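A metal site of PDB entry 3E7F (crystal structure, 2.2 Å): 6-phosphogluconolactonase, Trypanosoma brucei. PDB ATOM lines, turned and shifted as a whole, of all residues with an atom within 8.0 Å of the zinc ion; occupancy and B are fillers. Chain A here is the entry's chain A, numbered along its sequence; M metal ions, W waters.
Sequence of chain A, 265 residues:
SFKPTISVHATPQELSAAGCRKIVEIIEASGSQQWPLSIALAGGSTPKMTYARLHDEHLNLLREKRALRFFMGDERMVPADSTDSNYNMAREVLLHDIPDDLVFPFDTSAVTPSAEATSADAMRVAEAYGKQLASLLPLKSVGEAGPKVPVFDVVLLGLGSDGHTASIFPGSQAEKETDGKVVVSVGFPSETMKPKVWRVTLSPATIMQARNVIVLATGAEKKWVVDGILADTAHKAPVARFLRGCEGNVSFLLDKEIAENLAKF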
ATOM      1  N   HIS A  55      11.910  17.856 -19.952  1.00  0.00           N
ATOM      2  CA  HIS A  55      12.766  17.414 -21.054  1.00  0.00           C
ATOM      3  C   HIS A  55      12.218  16.161 -21.752  1.00  0.00           C
ATOM      4  O   HIS A  55      12.327  16.053 -22.975  1.00  0.00           O
ATOM      5  CB  HIS A  55      14.194  17.177 -20.579  1.00  0.00           C
ATOM      6  CG  HIS A  55      15.058  16.435 -21.572  1.00  0.00           C
ATOM      7  ND1 HIS A  55      14.926  15.084 -21.804  1.00  0.00           N
ATOM      8  CD2 HIS A  55      16.087  16.860 -22.346  1.00  0.00           C
ATOM      9  CE1 HIS A  55      15.844  14.701 -22.682  1.00  0.00           C
ATOM     10  NE2 HIS A  55      16.537  15.762 -23.044  1.00  0.00           N
ATOM     11  N   ASP A  56      11.649  15.241 -20.961  1.00  0.00           N
ATOM     12  CA  ASP A  56      11.153  13.929 -21.444  1.00  0.00           C
ATOM     13  C   ASP A  56       9.715  13.948 -21.963  1.00  0.00           C
ATOM     14  O   ASP A  56       9.302  13.123 -22.764  1.00  0.00           O
ATOM     15  CB  ASP A  56      11.232  12.851 -20.337  1.00  0.00           C
ATOM     16  CG  ASP A  56      12.662  12.525 -19.899  1.00  0.00           C
ATOM     17  OD1 ASP A  56      13.629  12.901 -20.595  1.00  0.00           O
ATOM     18  OD2 ASP A  56      12.818  11.896 -18.833  1.00  0.00           O
ATOM     19  N   LEU A  59       9.292  18.476 -24.396  1.00  0.00           N
ATOM     20  CA  LEU A  59      10.290  19.138 -25.203  1.00  0.00           C
ATOM     21  C   LEU A  59       9.645  19.935 -26.327  1.00  0.00           C
ATOM     22  O   LEU A  59      10.073  21.056 -26.649  1.00  0.00           O
ATOM     23  CB  LEU A  59      11.253  18.152 -25.834  1.00  0.00           C
ATOM     24  CG  LEU A  59      12.658  18.689 -26.066  1.00  0.00           C
ATOM     25  CD1 LEU A  59      13.360  18.104 -27.235  1.00  0.00           C
ATOM     26  CD2 LEU A  59      12.818  20.177 -25.956  1.00  0.00           C
ATOM     27  N   ARG A  63      10.640  23.664 -27.261  1.00  0.00           N
ATOM     28  CA  ARG A  63      11.547  23.822 -28.372  1.00  0.00           C
ATOM     29  C   ARG A  63      10.747  24.246 -29.599  1.00  0.00           C
ATOM     30  O   ARG A  63      10.775  25.407 -29.980  1.00  0.00           O
ATOM     31  CB  ARG A  63      12.250  22.502 -28.649  1.00  0.00           C
ATOM     32  CG  ARG A  63      13.315  22.612 -29.717  1.00  0.00           C
ATOM     33  CD  ARG A  63      14.033  21.303 -29.874  1.00  0.00           C
ATOM     34  NE  ARG A  63      13.108  20.257 -30.318  1.00  0.00           N
ATOM     35  CZ  ARG A  63      13.508  19.034 -30.602  1.00  0.00           C
ATOM     36  NH1 ARG A  63      14.792  18.744 -30.499  1.00  0.00           N
ATOM     37  NH2 ARG A  63      12.645  18.111 -31.019  1.00  0.00           N
ATOM     38  N   ARG A  91      21.223  22.695 -17.516  1.00  0.00           N
ATOM     39  CA  ARG A  91      21.611  22.381 -18.869  1.00  0.00           C
ATOM     40  C   ARG A  91      21.779  20.894 -19.117  1.00  0.00           C
ATOM     41  O   ARG A  91      21.426  20.384 -20.178  1.00  0.00           O
ATOM     42  CB  ARG A  91      22.894  23.071 -19.270  1.00  0.00           C
ATOM     43  CG  ARG A  91      23.195  22.834 -20.756  1.00  0.00           C
ATOM     44  CD  ARG A  91      24.622  23.210 -21.151  1.00  0.00           C
ATOM     45  NE  ARG A  91      24.963  22.551 -22.408  1.00  0.00           N
ATOM     46  CZ  ARG A  91      25.312  21.261 -22.525  1.00  0.00           C
ATOM     47  NH1 ARG A  91      25.578  20.756 -23.719  1.00  0.00           N
ATOM     48  NH2 ARG A  91      25.416  20.484 -21.438  1.00  0.00           N
ATOM     49  N   GLU A  92      22.359  20.205 -18.155  1.00  0.00           N
ATOM     50  CA  GLU A  92      22.544  18.782 -18.318  1.00  0.00           C
ATOM     51  C   GLU A  92      21.213  18.066 -18.520  1.00  0.00           C
ATOM     52  O   GLU A  92      21.095  17.200 -19.400  1.00  0.00           O
ATOM     53  CB  GLU A  92      23.338  18.181 -17.153  1.00  0.00           C
ATOM     54  CG  GLU A  92      23.114  16.679 -16.983  1.00  0.00           C
ATOM     55  CD  GLU A  92      23.871  16.110 -15.785  1.00  0.00           C
ATOM     56  OE1 GLU A  92      24.969  16.637 -15.481  1.00  0.00           O
ATOM     57  OE2 GLU A  92      23.382  15.124 -15.162  1.00  0.00           O
ATOM     58  N   VAL A  93      20.219  18.400 -17.714  1.00  0.00           N
ATOM     59  CA  VAL A  93      18.933  17.712 -17.795  1.00  0.00           C
ATOM     60  C   VAL A  93      17.918  18.252 -18.819  1.00  0.00           C
ATOM     61  O   VAL A  93      16.985  17.554 -19.188  1.00  0.00           O
ATOM     62  CB  VAL A  93      18.292  17.632 -16.383  1.00  0.00           C
ATOM     63  CG1 VAL A  93      17.880  19.003 -15.898  1.00  0.00           C
ATOM     64  CG2 VAL A  93      17.093  16.763 -16.418  1.00  0.00           C
ATOM     65  N   LEU A  94      18.006  19.516 -19.173  1.00  0.00           N
ATOM     66  CA  LEU A  94      16.976  20.078 -20.045  1.00  0.00           C
ATOM     67  C   LEU A  94      17.500  21.029 -21.093  1.00  0.00           C
ATOM     68  O   LEU A  94      17.215  20.882 -22.270  1.00  0.00           O
ATOM     69  CB  LEU A  94      15.915  20.786 -19.191  1.00  0.00           C
ATOM     70  CG  LEU A  94      14.920  21.715 -19.897  1.00  0.00           C
ATOM     71  CD1 LEU A  94      13.963  20.894 -20.797  1.00  0.00           C
ATOM     72  CD2 LEU A  94      14.137  22.447 -18.857  1.00  0.00           C
ATOM     73  N   LEU A  95      18.222  22.054 -20.665  1.00  0.00           N
ATOM     74  CA  LEU A  95      18.620  23.127 -21.572  1.00  0.00           C
ATOM     75  C   LEU A  95      19.527  22.847 -22.763  1.00  0.00           C
ATOM     76  O   LEU A  95      19.688  23.718 -23.639  1.00  0.00           O
ATOM     77  CB  LEU A  95      19.088  24.361 -20.784  1.00  0.00           C
ATOM     78  CG  LEU A  95      18.277  24.832 -19.571  1.00  0.00           C
ATOM     79  CD1 LEU A  95      19.021  26.027 -18.861  1.00  0.00           C
ATOM     80  CD2 LEU A  95      16.823  25.204 -19.935  1.00  0.00           C
ATOM     81  N   HIS A  96      20.213  21.712 -22.777  1.00  0.00           N
ATOM     82  CA  HIS A  96      21.112  21.419 -23.909  1.00  0.00           C
ATOM     83  C   HIS A  96      20.202  21.282 -25.173  1.00  0.00           C
ATOM     84  O   HIS A  96      20.689  21.336 -26.292  1.00  0.00           O
ATOM     85  CB  HIS A  96      21.839  20.101 -23.656  1.00  0.00           C
ATOM     86  CG  HIS A  96      20.917  18.953 -23.355  1.00  0.00           C
ATOM     87  ND1 HIS A  96      20.400  18.732 -22.096  1.00  0.00           N
ATOM     88  CD2 HIS A  96      20.354  18.031 -24.169  1.00  0.00           C
ATOM     89  CE1 HIS A  96      19.615  17.666 -22.134  1.00  0.00           C
ATOM     90  NE2 HIS A  96      19.545  17.244 -23.385  1.00  0.00           N
ATOM     91  N   ASP A  97      18.889  21.119 -24.946  1.00  0.00           N
ATOM     92  CA  ASP A  97      17.873  20.957 -25.998  1.00  0.00           C
ATOM     93  C   ASP A  97      17.009  22.207 -26.264  1.00  0.00           C
ATOM     94  O   ASP A  97      16.162  22.222 -27.168  1.00  0.00           O
ATOM     95  CB  ASP A  97      16.942  19.805 -25.618  1.00  0.00           C
ATOM     96  CG  ASP A  97      17.531  18.458 -25.945  1.00  0.00           C
ATOM     97  OD1 ASP A  97      17.215  17.472 -25.245  1.00  0.00           O
ATOM     98  OD2 ASP A  97      18.377  18.426 -26.857  1.00  0.00           O
ATOM     99  N   ILE A  98      17.179  23.245 -25.463  1.00  0.00           N
ATOM    100  CA  ILE A  98      16.417  24.490 -25.631  1.00  0.00           C
ATOM    101  C   ILE A  98      17.160  25.483 -26.550  1.00  0.00           C
ATOM    102  O   ILE A  98      18.375  25.691 -26.421  1.00  0.00           O
ATOM    103  CB  ILE A  98      16.078  25.141 -24.265  1.00  0.00           C
ATOM    104  CG1 ILE A  98      15.495  24.108 -23.272  1.00  0.00           C
ATOM    105  CG2 ILE A  98      15.182  26.348 -24.443  1.00  0.00           C
ATOM    106  CD1 ILE A  98      14.268  23.413 -23.756  1.00  0.00           C
HETATM  107 ZN    ZN M   1      18.133  16.039 -24.281  1.00  0.00          ZN
HETATM  108  O   HOH W   1      19.057  14.285 -22.458  1.00  0.00           O
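The zinc ion is bound by OD1 of Asp 97, NE2 of His 55 and NE2 of His 96. The zinc ion has three donor atoms within binding distance. Slightly farther from the zinc ion lies water W1 (2.7 Å).
The side-chain carboxylate (OD1) of Asp 56 sits at hydrogen-bond distance from a ring nitrogen (ND1) of His 55, 2.8 Å away. A ring nitrogen (ND1) of His 96 lies close to the backbone carbonyl oxygen (O) of Glu 92 (3.2 Å). The backbone carbonyl oxygen (O) of Arg 91 lies within hydrogen-bond range of a ring nitrogen (ND1) of His 96 (2.7 Å).
Within 4 Å of the zinc ion: His 55, His 96 and Asp 97. The nearest printed residue that does not touch the zinc ion is Leu 94 (5.3 Å).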
